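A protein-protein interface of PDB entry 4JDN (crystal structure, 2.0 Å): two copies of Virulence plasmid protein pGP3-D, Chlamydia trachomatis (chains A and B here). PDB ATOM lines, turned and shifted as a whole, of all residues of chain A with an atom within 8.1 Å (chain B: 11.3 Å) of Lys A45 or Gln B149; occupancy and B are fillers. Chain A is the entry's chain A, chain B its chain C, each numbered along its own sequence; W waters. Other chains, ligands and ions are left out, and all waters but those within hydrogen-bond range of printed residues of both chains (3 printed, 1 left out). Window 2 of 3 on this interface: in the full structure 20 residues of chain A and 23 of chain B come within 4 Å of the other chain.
No residue of chain B comes within 4 Å of Lys A6. Of chain B, only Gln B149 comes within 4 Å of Ala A7. Printed residues of chain B within 4 Å of Asn A10: Ser B98 (3.4 Å). Thr A43 touches just one residue of chain B: Gln B149 (2.8 Å). Of chain B, only Gln B149 (3.0 Å) comes within 4 Å of Lys A45. No residue of chain B comes within 4 Å of Ser A46. No residue of chain B comes within 4 Å of Ser A47. Ile A147 touches none of the printed residues of chain B. Of the printed residues of chain A, Ser B98 touches Phe A8 (3.999 Å) and Asn A10 (3.4 Å). Of the printed residues of chain A, Val B146 touches Phe A8 (3.6 Å). Of the printed residues of chain A, Ile B147 touches Phe A8. Of chain A, only Ala A7 (3.3 Å), Phe A8 (2.8 Å), Asn A9 (3.1 Å), Thr A43 (2.8 Å) and Lys A45 (3.0 Å) come within 4 Å of Gln B149. The nearest printed residue of chain A that does not touch Ser B98 is Asn A9 (6.3 Å).
N of Glu A145 lies within hydrogen-bond range of O of Ala A7. O of Asn A9 is in hydrogen-bond range of N of Phe A143 (2.9 Å). The backbone NH (N) of Lys A45 lies within hydrogen-bond range of the side-chain carboxylate (OE1) of Glu A145, at 2.8 Å. N of Met B50 is in hydrogen-bond range of O of Val B146 (2.8 Å). The side-chain amide nitrogen of Gln B149 sits at hydrogen-bond distance from the side-chain amide oxygen of Asn B151.
CB of Ala A7 touches OE1 of Gln B149 (3.3 Å). SD of Met B50 touches CE2 of Phe A8, 3.7 Å away. CZ of Phe A8 touches OG of Ser B98, at 3.999 Å. CG2 of Val B146 touches CD2 of Phe A8, 3.6 Å away. Phe A8 touches Ile B147 (CB to O, 3.8 Å). Phe A8 touches Pro B148 (O to CA, 3.2 Å). CG of Asn A10 touches OG of Ser B98 (3.4 Å).
Water W3 lies within hydrogen-bond range of NE2 of Gln B149 (2.6 Å), OD1 of Asn A9 (2.8 Å), N of Thr A43 (2.9 Å) and OD1 of Asn B151 (3.5 Å). Water W1 lies within hydrogen-bond range of the side-chain hydroxyl (OG1) of Thr A43 (2.8 Å), the backbone carbonyl oxygen (O) of Thr A41 (3.1 Å) and the side-chain amide oxygen (OD1) of Asn B151 (3.4 Å). Water W2 lies within hydrogen-bond range of the side-chain amide oxygen (OD1) of Asn A10 and the side-chain hydroxyl (OG) of Ser B98.
Of the 24 printed residues of chain A, 6 touch a printed residue of chain B. Hydrophobic or aromatic side chains of chain A that line the printed part of chain B: Ala A7 and Phe A8.
Positions printed for both chains: 6, 47, 48, 49, 145 and 147. Of the 12 pairs that touch across the chains among the printed residues, none has its exchanged pair printed and touching as well.
N of Gln B149 is in hydrogen-bond range of O of Phe A8, at 2.8 Å. ND2 of Asn A9 is in hydrogen-bond range of O of Gln B149 (3.1 Å). The side-chain amide oxygen of Asn A9 lies close to the side-chain amide oxygen of Asn B151 (3.1 Å). O of Thr A43 lies close to OE1 of Gln B149, at 2.8 Å. The side-chain amide oxygen (OE1) of Gln B149 sits at hydrogen-bond distance from the side-chain amino group (NZ) of Lys A45, 3.0 Å away.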
ATOM      1  N   LYS A   6      33.621   2.322  10.974  1.00  0.00           N
ATOM      2  CA  LYS A   6      32.308   1.950  10.460  1.00  0.00           C
ATOM      3  C   LYS A   6      31.621   3.154   9.819  1.00  0.00           C
ATOM      4  O   LYS A   6      31.704   4.276  10.314  1.00  0.00           O
ATOM      5  CB  LYS A   6      31.426   1.340  11.561  1.00  0.00           C
ATOM      6  CG  LYS A   6      31.920  -0.018  12.084  1.00  0.00           C
ATOM      7  CD  LYS A   6      33.018   0.157  13.126  1.00  0.00           C
ATOM      8  CE  LYS A   6      34.138  -0.858  12.951  1.00  0.00           C
ATOM      9  NZ  LYS A   6      35.333  -0.496  13.776  1.00  0.00           N
ATOM     10  N   ALA A   7      30.945   2.906   8.708  1.00  0.00           N
ATOM     11  CA  ALA A   7      30.316   3.968   7.943  1.00  0.00           C
ATOM     12  C   ALA A   7      29.012   4.439   8.590  1.00  0.00           C
ATOM     13  O   ALA A   7      28.217   3.630   9.077  1.00  0.00           O
ATOM     14  CB  ALA A   7      30.055   3.491   6.525  1.00  0.00           C
ATOM     15  N   PHE A   8      28.817   5.754   8.613  1.00  0.00           N
ATOM     16  CA  PHE A   8      27.500   6.336   8.830  1.00  0.00           C
ATOM     17  C   PHE A   8      27.267   7.459   7.818  1.00  0.00           C
ATOM     18  O   PHE A   8      28.173   8.249   7.537  1.00  0.00           O
ATOM     19  CB  PHE A   8      27.339   6.914  10.237  1.00  0.00           C
ATOM     20  CG  PHE A   8      26.028   7.644  10.420  1.00  0.00           C
ATOM     21  CD1 PHE A   8      24.866   6.939  10.692  1.00  0.00           C
ATOM     22  CD2 PHE A   8      25.947   9.015  10.257  1.00  0.00           C
ATOM     23  CE1 PHE A   8      23.651   7.593  10.824  1.00  0.00           C
ATOM     24  CE2 PHE A   8      24.732   9.679  10.386  1.00  0.00           C
ATOM     25  CZ  PHE A   8      23.585   8.970  10.677  1.00  0.00           C
ATOM     26  N   ASN A   9      26.047   7.551   7.299  1.00  0.00           N
ATOM     27  CA  ASN A   9      25.654   8.694   6.475  1.00  0.00           C
ATOM     28  C   ASN A   9      24.167   8.952   6.643  1.00  0.00           C
ATOM     29  O   ASN A   9      23.372   8.015   6.715  1.00  0.00           O
ATOM     30  CB  ASN A   9      25.939   8.455   4.979  1.00  0.00           C
ATOM     31  CG  ASN A   9      27.412   8.632   4.610  1.00  0.00           C
ATOM     32  OD1 ASN A   9      28.047   7.698   4.128  1.00  0.00           O
ATOM     33  ND2 ASN A   9      27.951   9.826   4.828  1.00  0.00           N
ATOM     34  N   ASN A  10      23.807  10.227   6.698  1.00  0.00           N
ATOM     35  CA  ASN A  10      22.415  10.626   6.640  1.00  0.00           C
ATOM     36  C   ASN A  10      22.098  11.396   5.373  1.00  0.00           C
ATOM     37  O   ASN A  10      22.895  12.221   4.911  1.00  0.00           O
ATOM     38  CB  ASN A  10      22.035  11.478   7.841  1.00  0.00           C
ATOM     39  CG  ASN A  10      20.564  11.797   7.846  1.00  0.00           C
ATOM     40  OD1 ASN A  10      19.731  10.891   7.920  1.00  0.00           O
ATOM     41  ND2 ASN A  10      20.231  13.066   7.707  1.00  0.00           N
ATOM     42  N   PHE A  11      20.925  11.132   4.815  1.00  0.00           N
ATOM     43  CA  PHE A  11      20.525  11.754   3.566  1.00  0.00           C
ATOM     44  C   PHE A  11      19.167  12.436   3.741  1.00  0.00           C
ATOM     45  O   PHE A  11      18.130  11.779   3.711  1.00  0.00           O
ATOM     46  CB  PHE A  11      20.471  10.713   2.434  1.00  0.00           C
ATOM     47  CG  PHE A  11      21.762   9.965   2.236  1.00  0.00           C
ATOM     48  CD1 PHE A  11      22.755  10.468   1.409  1.00  0.00           C
ATOM     49  CD2 PHE A  11      21.981   8.747   2.885  1.00  0.00           C
ATOM     50  CE1 PHE A  11      23.947   9.783   1.231  1.00  0.00           C
ATOM     51  CE2 PHE A  11      23.167   8.052   2.718  1.00  0.00           C
ATOM     52  CZ  PHE A  11      24.152   8.562   1.886  1.00  0.00           C
ATOM     53  N   THR A  41      24.504   6.359  -1.991  1.00  0.00           N
ATOM     54  CA  THR A  41      25.642   5.461  -2.173  1.00  0.00           C
ATOM     55  C   THR A  41      26.448   5.380  -0.891  1.00  0.00           C
ATOM     56  O   THR A  41      26.932   6.391  -0.386  1.00  0.00           O
ATOM     57  CB  THR A  41      26.539   5.913  -3.347  1.00  0.00           C
ATOM     58  OG1 THR A  41      25.769   5.876  -4.554  1.00  0.00           O
ATOM     59  CG2 THR A  41      27.765   4.991  -3.491  1.00  0.00           C
ATOM     60  N   VAL A  42      26.558   4.175  -0.344  1.00  0.00           N
ATOM     61  CA  VAL A  42      27.272   3.984   0.907  1.00  0.00           C
ATOM     62  C   VAL A  42      28.355   2.929   0.719  1.00  0.00           C
ATOM     63  O   VAL A  42      28.233   2.047  -0.132  1.00  0.00           O
ATOM     64  CB  VAL A  42      26.327   3.578   2.064  1.00  0.00           C
ATOM     65  CG1 VAL A  42      25.434   4.767   2.476  1.00  0.00           C
ATOM     66  CG2 VAL A  42      25.486   2.382   1.654  1.00  0.00           C
ATOM     67  N   THR A  43      29.412   3.025   1.513  1.00  0.00           N
ATOM     68  CA  THR A  43      30.546   2.113   1.383  1.00  0.00           C
ATOM     69  C   THR A  43      30.903   1.524   2.735  1.00  0.00           C
ATOM     70  O   THR A  43      31.345   2.246   3.620  1.00  0.00           O
ATOM     71  CB  THR A  43      31.798   2.844   0.895  1.00  0.00           C
ATOM     72  OG1 THR A  43      31.479   3.648  -0.248  1.00  0.00           O
ATOM     73  CG2 THR A  43      32.893   1.824   0.540  1.00  0.00           C
ATOM     74  N   PRO A  44      30.707   0.210   2.900  1.00  0.00           N
ATOM     75  CA  PRO A  44      31.046  -0.404   4.188  1.00  0.00           C
ATOM     76  C   PRO A  44      32.548  -0.353   4.426  1.00  0.00           C
ATOM     77  O   PRO A  44      33.320  -0.465   3.473  1.00  0.00           O
ATOM     78  CB  PRO A  44      30.541  -1.848   4.049  1.00  0.00           C
ATOM     79  CG  PRO A  44      30.262  -2.050   2.598  1.00  0.00           C
ATOM     80  CD  PRO A  44      30.011  -0.710   1.987  1.00  0.00           C
ATOM     81  N   LYS A  45      32.956  -0.147   5.672  1.00  0.00           N
ATOM     82  CA  LYS A  45      34.373  -0.138   6.019  1.00  0.00           C
ATOM     83  C   LYS A  45      34.750  -1.497   6.577  1.00  0.00           C
ATOM     84  O   LYS A  45      35.923  -1.813   6.749  1.00  0.00           O
ATOM     85  CB  LYS A  45      34.660   0.907   7.087  1.00  0.00           C
ATOM     86  CG  LYS A  45      34.478   2.365   6.678  1.00  0.00           C
ATOM     87  CD  LYS A  45      34.740   3.258   7.906  1.00  0.00           C
ATOM     88  CE  LYS A  45      34.830   4.751   7.559  1.00  0.00           C
ATOM     89  NZ  LYS A  45      33.510   5.340   7.181  1.00  0.00           N
ATOM     90  N   SER A  46      33.739  -2.293   6.896  1.00  0.00           N
ATOM     91  CA  SER A  46      33.985  -3.591   7.487  1.00  0.00           C
ATOM     92  C   SER A  46      33.355  -4.703   6.675  1.00  0.00           C
ATOM     93  O   SER A  46      32.209  -4.602   6.241  1.00  0.00           O
ATOM     94  CB  SER A  46      33.462  -3.640   8.914  1.00  0.00           C
ATOM     95  OG  SER A  46      33.283  -4.993   9.277  1.00  0.00           O
ATOM     96  N   SER A  47      34.103  -5.774   6.467  1.00  0.00           N
ATOM     97  CA  SER A  47      33.559  -6.926   5.764  1.00  0.00           C
ATOM     98  C   SER A  47      32.596  -7.653   6.700  1.00  0.00           C
ATOM     99  O   SER A  47      32.787  -7.660   7.912  1.00  0.00           O
ATOM    100  CB  SER A  47      34.692  -7.854   5.326  1.00  0.00           C
ATOM    101  OG  SER A  47      35.294  -8.466   6.450  1.00  0.00           O
ATOM    102  N   GLY A  48      31.550  -8.252   6.144  1.00  0.00           N
ATOM    103  CA  GLY A  48      30.605  -9.012   6.947  1.00  0.00           C
ATOM    104  C   GLY A  48      29.755  -8.184   7.898  1.00  0.00           C
ATOM    105  O   GLY A  48      29.166  -8.714   8.848  1.00  0.00           O
ATOM    106  N   SER A  49      29.691  -6.879   7.653  1.00  0.00           N
ATOM    107  CA  SER A  49      28.855  -5.999   8.463  1.00  0.00           C
ATOM    108  C   SER A  49      27.427  -5.925   7.922  1.00  0.00           C
ATOM    109  O   SER A  49      27.076  -6.578   6.937  1.00  0.00           O
ATOM    110  CB  SER A  49      29.444  -4.590   8.478  1.00  0.00           C
ATOM    111  OG  SER A  49      29.409  -4.038   7.169  1.00  0.00           O
ATOM    112  N   PHE A  51      24.089  -2.790   7.441  1.00  0.00           N
ATOM    113  CA  PHE A  51      23.686  -1.396   7.572  1.00  0.00           C
ATOM    114  C   PHE A  51      22.334  -1.380   8.272  1.00  0.00           C
ATOM    115  O   PHE A  51      21.385  -2.040   7.842  1.00  0.00           O
ATOM    116  CB  PHE A  51      23.549  -0.707   6.214  1.00  0.00           C
ATOM    117  CG  PHE A  51      24.839  -0.117   5.690  1.00  0.00           C
ATOM    118  CD1 PHE A  51      25.466   0.925   6.360  1.00  0.00           C
ATOM    119  CD2 PHE A  51      25.398  -0.588   4.511  1.00  0.00           C
ATOM    120  CE1 PHE A  51      26.650   1.476   5.867  1.00  0.00           C
ATOM    121  CE2 PHE A  51      26.579  -0.051   4.019  1.00  0.00           C
ATOM    122  CZ  PHE A  51      27.205   0.983   4.703  1.00  0.00           C
ATOM    123  N   ASN A 101      25.947  -6.597   4.209  1.00  0.00           N
ATOM    124  CA  ASN A 101      26.907  -6.079   3.250  1.00  0.00           C
ATOM    125  C   ASN A 101      27.782  -7.186   2.679  1.00  0.00           C
ATOM    126  O   ASN A 101      28.153  -8.118   3.389  1.00  0.00           O
ATOM    127  CB  ASN A 101      27.774  -5.014   3.921  1.00  0.00           C
ATOM    128  CG  ASN A 101      26.969  -3.814   4.349  1.00  0.00           C
ATOM    129  OD1 ASN A 101      26.054  -3.399   3.634  1.00  0.00           O
ATOM    130  ND2 ASN A 101      27.275  -3.263   5.524  1.00  0.00           N
ATOM    131  N   GLY A 103      31.306  -7.287   1.127  1.00  0.00           N
ATOM    132  CA  GLY A 103      32.558  -6.665   0.744  1.00  0.00           C
ATOM    133  C   GLY A 103      32.575  -5.169   0.972  1.00  0.00           C
ATOM    134  O   GLY A 103      31.722  -4.633   1.680  1.00  0.00           O
ATOM    135  N   LEU A 104      33.539  -4.499   0.346  1.00  0.00           N
ATOM    136  CA  LEU A 104      33.873  -3.112   0.659  1.00  0.00           C
ATOM    137  C   LEU A 104      33.630  -2.122  -0.488  1.00  0.00           C
ATOM    138  O   LEU A 104      34.078  -0.989  -0.432  1.00  0.00           O
ATOM    139  CB  LEU A 104      35.342  -3.041   1.066  1.00  0.00           C
ATOM    140  CG  LEU A 104      35.659  -2.583   2.482  1.00  0.00           C
ATOM    141  CD1 LEU A 104      34.970  -3.480   3.505  1.00  0.00           C
ATOM    142  CD2 LEU A 104      37.183  -2.504   2.707  1.00  0.00           C
ATOM    143  N   THR A 105      32.941  -2.544  -1.535  1.00  0.00           N
ATOM    144  CA  THR A 105      32.681  -1.645  -2.650  1.00  0.00           C
ATOM    145  C   THR A 105      31.476  -0.754  -2.356  1.00  0.00           C
ATOM    146  O   THR A 105      30.563  -1.160  -1.635  1.00  0.00           O
ATOM    147  CB  THR A 105      32.443  -2.438  -3.937  1.00  0.00           C
ATOM    148  OG1 THR A 105      31.743  -3.640  -3.610  1.00  0.00           O
ATOM    149  CG2 THR A 105      33.770  -2.814  -4.571  1.00  0.00           C
ATOM    150  N   PRO A 106      31.481   0.473  -2.899  1.00  0.00           N
ATOM    151  CA  PRO A 106      30.320   1.360  -2.762  1.00  0.00           C
ATOM    152  C   PRO A 106      29.077   0.672  -3.299  1.00  0.00           C
ATOM    153  O   PRO A 106      29.127   0.024  -4.340  1.00  0.00           O
ATOM    154  CB  PRO A 106      30.671   2.551  -3.657  1.00  0.00           C
ATOM    155  CG  PRO A 106      32.162   2.506  -3.790  1.00  0.00           C
ATOM    156  CD  PRO A 106      32.548   1.069  -3.724  1.00  0.00           C
ATOM    157  N   PHE A 143      21.971   5.503   7.196  1.00  0.00           N
ATOM    158  CA  PHE A 143      22.624   4.212   7.064  1.00  0.00           C
ATOM    159  C   PHE A 143      23.715   4.175   8.129  1.00  0.00           C
ATOM    160  O   PHE A 143      24.621   5.018   8.115  1.00  0.00           O
ATOM    161  CB  PHE A 143      23.294   4.086   5.692  1.00  0.00           C
ATOM    162  CG  PHE A 143      22.332   3.925   4.540  1.00  0.00           C
ATOM    163  CD1 PHE A 143      21.619   5.017   4.047  1.00  0.00           C
ATOM    164  CD2 PHE A 143      22.160   2.691   3.940  1.00  0.00           C
ATOM    165  CE1 PHE A 143      20.748   4.869   2.968  1.00  0.00           C
ATOM    166  CE2 PHE A 143      21.275   2.526   2.871  1.00  0.00           C
ATOM    167  CZ  PHE A 143      20.569   3.625   2.384  1.00  0.00           C
ATOM    168  N   GLU A 145      26.526   1.598   9.820  1.00  0.00           N
ATOM    169  CA  GLU A 145      27.184   0.312   9.675  1.00  0.00           C
ATOM    170  C   GLU A 145      27.420  -0.289  11.051  1.00  0.00           C
ATOM    171  O   GLU A 145      27.902   0.390  11.959  1.00  0.00           O
ATOM    172  CB  GLU A 145      28.500   0.432   8.900  1.00  0.00           C
ATOM    173  CG  GLU A 145      29.219  -0.915   8.715  1.00  0.00           C
ATOM    174  CD  GLU A 145      30.467  -0.816   7.846  1.00  0.00           C
ATOM    175  OE1 GLU A 145      30.985   0.312   7.653  1.00  0.00           O
ATOM    176  OE2 GLU A 145      30.917  -1.872   7.350  1.00  0.00           O
ATOM    177  N   ILE A 147      28.362  -4.238  13.255  1.00  0.00           N
ATOM    178  CA  ILE A 147      28.849  -5.616  13.200  1.00  0.00           C
ATOM    179  C   ILE A 147      27.921  -6.532  13.984  1.00  0.00           C
ATOM    180  O   ILE A 147      27.779  -6.380  15.190  1.00  0.00           O
ATOM    181  CB  ILE A 147      30.244  -5.724  13.818  1.00  0.00           C
ATOM    182  CG1 ILE A 147      31.173  -4.677  13.203  1.00  0.00           C
ATOM    183  CG2 ILE A 147      30.803  -7.126  13.621  1.00  0.00           C
ATOM    184  CD1 ILE A 147      31.584  -5.018  11.810  1.00  0.00           C
ATOM    185  N   LYS B   6      32.073   7.656  21.422  1.00  0.00           N
ATOM    186  CA  LYS B   6      31.463   8.983  21.503  1.00  0.00           C
ATOM    187  C   LYS B   6      30.366   9.032  22.562  1.00  0.00           C
ATOM    188  O   LYS B   6      30.503   8.467  23.646  1.00  0.00           O
ATOM    189  CB  LYS B   6      30.888   9.411  20.150  1.00  0.00           C
ATOM    190  CG  LYS B   6      31.902   9.547  19.005  1.00  0.00           C
ATOM    191  CD  LYS B   6      32.158   8.196  18.349  1.00  0.00           C
ATOM    192  CE  LYS B   6      30.883   7.353  18.325  1.00  0.00           C
ATOM    193  NZ  LYS B   6      31.137   5.969  17.833  1.00  0.00           N
ATOM    194  N   SER B  47      34.893  16.184  17.461  1.00  0.00           N
ATOM    195  CA  SER B  47      34.851  17.218  16.439  1.00  0.00           C
ATOM    196  C   SER B  47      34.302  16.615  15.167  1.00  0.00           C
ATOM    197  O   SER B  47      34.593  15.458  14.848  1.00  0.00           O
ATOM    198  CB  SER B  47      36.258  17.763  16.169  1.00  0.00           C
ATOM    199  OG  SER B  47      36.801  18.373  17.325  1.00  0.00           O
ATOM    200  N   GLY B  48      33.499  17.389  14.444  1.00  0.00           N
ATOM    201  CA  GLY B  48      32.996  16.955  13.146  1.00  0.00           C
ATOM    202  C   GLY B  48      31.968  15.827  13.182  1.00  0.00           C
ATOM    203  O   GLY B  48      31.745  15.142  12.180  1.00  0.00           O
ATOM    204  N   SER B  49      31.348  15.618  14.333  1.00  0.00           N
ATOM    205  CA  SER B  49      30.381  14.539  14.474  1.00  0.00           C
ATOM    206  C   SER B  49      28.963  15.032  14.216  1.00  0.00           C
ATOM    207  O   SER B  49      28.737  16.233  14.049  1.00  0.00           O
ATOM    208  CB  SER B  49      30.460  13.936  15.882  1.00  0.00           C
ATOM    209  OG  SER B  49      29.964  14.839  16.855  1.00  0.00           O
ATOM    210  N   MET B  50      28.026  14.084  14.171  1.00  0.00           N
ATOM    211  CA  MET B  50      26.592  14.366  14.117  1.00  0.00           C
ATOM    212  C   MET B  50      25.891  13.810  15.351  1.00  0.00           C
ATOM    213  O   MET B  50      26.300  12.785  15.877  1.00  0.00           O
ATOM    214  CB  MET B  50      25.951  13.694  12.898  1.00  0.00           C
ATOM    215  CG  MET B  50      26.326  14.298  11.559  1.00  0.00           C
ATOM    216  SD  MET B  50      25.488  13.309  10.098  1.00  0.00           S
ATOM    217  CE  MET B  50      25.863  14.540   8.634  1.00  0.00           C
ATOM    218  N   SER B  98      19.402  14.427  11.980  1.00  0.00           N
ATOM    219  CA  SER B  98      20.834  14.304  12.179  1.00  0.00           C
ATOM    220  C   SER B  98      21.404  15.710  12.216  1.00  0.00           C
ATOM    221  O   SER B  98      21.401  16.419  11.211  1.00  0.00           O
ATOM    222  CB  SER B  98      21.483  13.499  11.045  1.00  0.00           C
ATOM    223  OG  SER B  98      21.157  12.115  11.128  1.00  0.00           O
ATOM    224  N   THR B 100      24.413  18.388  12.563  1.00  0.00           N
ATOM    225  CA  THR B 100      25.860  18.566  12.480  1.00  0.00           C
ATOM    226  C   THR B 100      26.334  19.339  13.722  1.00  0.00           C
ATOM    227  O   THR B 100      25.843  20.425  14.005  1.00  0.00           O
ATOM    228  CB  THR B 100      26.293  19.308  11.174  1.00  0.00           C
ATOM    229  OG1 THR B 100      26.104  18.459  10.032  1.00  0.00           O
ATOM    230  CG2 THR B 100      27.758  19.692  11.251  1.00  0.00           C
ATOM    231  N   GLU B 145      25.745  10.168  19.200  1.00  0.00           N
ATOM    232  CA  GLU B 145      26.804  10.838  18.447  1.00  0.00           C
ATOM    233  C   GLU B 145      27.501   9.867  17.493  1.00  0.00           C
ATOM    234  O   GLU B 145      27.960   8.803  17.901  1.00  0.00           O
ATOM    235  CB  GLU B 145      27.813  11.503  19.393  1.00  0.00           C
ATOM    236  CG  GLU B 145      28.879  12.333  18.678  1.00  0.00           C
ATOM    237  CD  GLU B 145      29.781  13.105  19.641  1.00  0.00           C
ATOM    238  OE1 GLU B 145      29.679  12.889  20.875  1.00  0.00           O
ATOM    239  OE2 GLU B 145      30.584  13.939  19.163  1.00  0.00           O
ATOM    240  N   VAL B 146      27.559  10.224  16.213  1.00  0.00           N
ATOM    241  CA  VAL B 146      28.183   9.366  15.209  1.00  0.00           C
ATOM    242  C   VAL B 146      29.118  10.197  14.326  1.00  0.00           C
ATOM    243  O   VAL B 146      28.928  11.402  14.179  1.00  0.00           O
ATOM    244  CB  VAL B 146      27.122   8.684  14.313  1.00  0.00           C
ATOM    245  CG1 VAL B 146      26.338   7.631  15.090  1.00  0.00           C
ATOM    246  CG2 VAL B 146      26.164   9.724  13.741  1.00  0.00           C
ATOM    247  N   ILE B 147      30.119   9.552  13.739  1.00  0.00           N
ATOM    248  CA  ILE B 147      31.000  10.212  12.775  1.00  0.00           C
ATOM    249  C   ILE B 147      30.575   9.849  11.361  1.00  0.00           C
ATOM    250  O   ILE B 147      30.649   8.681  10.971  1.00  0.00           O
ATOM    251  CB  ILE B 147      32.488   9.776  12.950  1.00  0.00           C
ATOM    252  CG1 ILE B 147      32.934   9.938  14.403  1.00  0.00           C
ATOM    253  CG2 ILE B 147      33.392  10.578  12.010  1.00  0.00           C
ATOM    254  CD1 ILE B 147      32.819  11.336  14.919  1.00  0.00           C
ATOM    255  N   PRO B 148      30.120  10.844  10.583  1.00  0.00           N
ATOM    256  CA  PRO B 148      29.684  10.563   9.215  1.00  0.00           C
ATOM    257  C   PRO B 148      30.872  10.260   8.311  1.00  0.00           C
ATOM    258  O   PRO B 148      31.931  10.849   8.501  1.00  0.00           O
ATOM    259  CB  PRO B 148      29.013  11.868   8.783  1.00  0.00           C
ATOM    260  CG  PRO B 148      29.636  12.919   9.636  1.00  0.00           C
ATOM    261  CD  PRO B 148      29.932  12.261  10.954  1.00  0.00           C
ATOM    262  N   GLN B 149      30.686   9.357   7.356  1.00  0.00           N
ATOM    263  CA  GLN B 149      31.757   8.909   6.473  1.00  0.00           C
ATOM    264  C   GLN B 149      31.980   9.854   5.308  1.00  0.00           C
ATOM    265  O   GLN B 149      31.029  10.233   4.618  1.00  0.00           O
ATOM    266  CB  GLN B 149      31.464   7.524   5.891  1.00  0.00           C
ATOM    267  CG  GLN B 149      32.516   7.122   4.839  1.00  0.00           C
ATOM    268  CD  GLN B 149      32.164   5.873   4.048  1.00  0.00           C
ATOM    269  OE1 GLN B 149      32.344   4.747   4.526  1.00  0.00           O
ATOM    270  NE2 GLN B 149      31.681   6.065   2.813  1.00  0.00           N
ATOM    271  N   THR B 150      33.238  10.219   5.082  1.00  0.00           N
ATOM    272  CA  THR B 150      33.590  10.969   3.885  1.00  0.00           C
ATOM    273  C   THR B 150      33.477  10.036   2.674  1.00  0.00           C
ATOM    274  O   THR B 150      34.121   8.980   2.626  1.00  0.00           O
ATOM    275  CB  THR B 150      34.998  11.575   3.999  1.00  0.00           C
ATOM    276  OG1 THR B 150      35.001  12.589   5.023  1.00  0.00           O
ATOM    277  CG2 THR B 150      35.437  12.183   2.661  1.00  0.00           C
ATOM    278  N   ASN B 151      32.639  10.404   1.708  1.00  0.00           N
ATOM    279  CA  ASN B 151      32.391   9.533   0.555  1.00  0.00           C
ATOM    280  C   ASN B 151      33.399   9.759  -0.579  1.00  0.00           C
ATOM    281  O   ASN B 151      33.571  10.880  -1.054  1.00  0.00           O
ATOM    282  CB  ASN B 151      30.948   9.698   0.037  1.00  0.00           C
ATOM    283  CG  ASN B 151      29.900   9.425   1.114  1.00  0.00           C
ATOM    284  OD1 ASN B 151      29.993   8.457   1.887  1.00  0.00           O
ATOM    285  ND2 ASN B 151      28.908  10.281   1.173  1.00  0.00           N
ATOM    286  N   ALA B 152      34.048   8.681  -1.011  1.00  0.00           N
ATOM    287  CA  ALA B 152      35.085   8.759  -2.040  1.00  0.00           C
ATOM    288  C   ALA B 152      34.481   9.066  -3.405  1.00  0.00           C
ATOM    289  O   ALA B 152      33.342   8.689  -3.670  1.00  0.00           O
ATOM    290  CB  ALA B 152      35.891   7.448  -2.093  1.00  0.00           C
HETATM  291  O   HOH W   1      29.978   5.969  -0.489  1.00  0.00           O
HETATM  292  O   HOH W   2      18.374  11.266  10.421  1.00  0.00           O
HETATM  293  O   HOH W   3      29.224   5.355   3.214  1.00  0.00           O
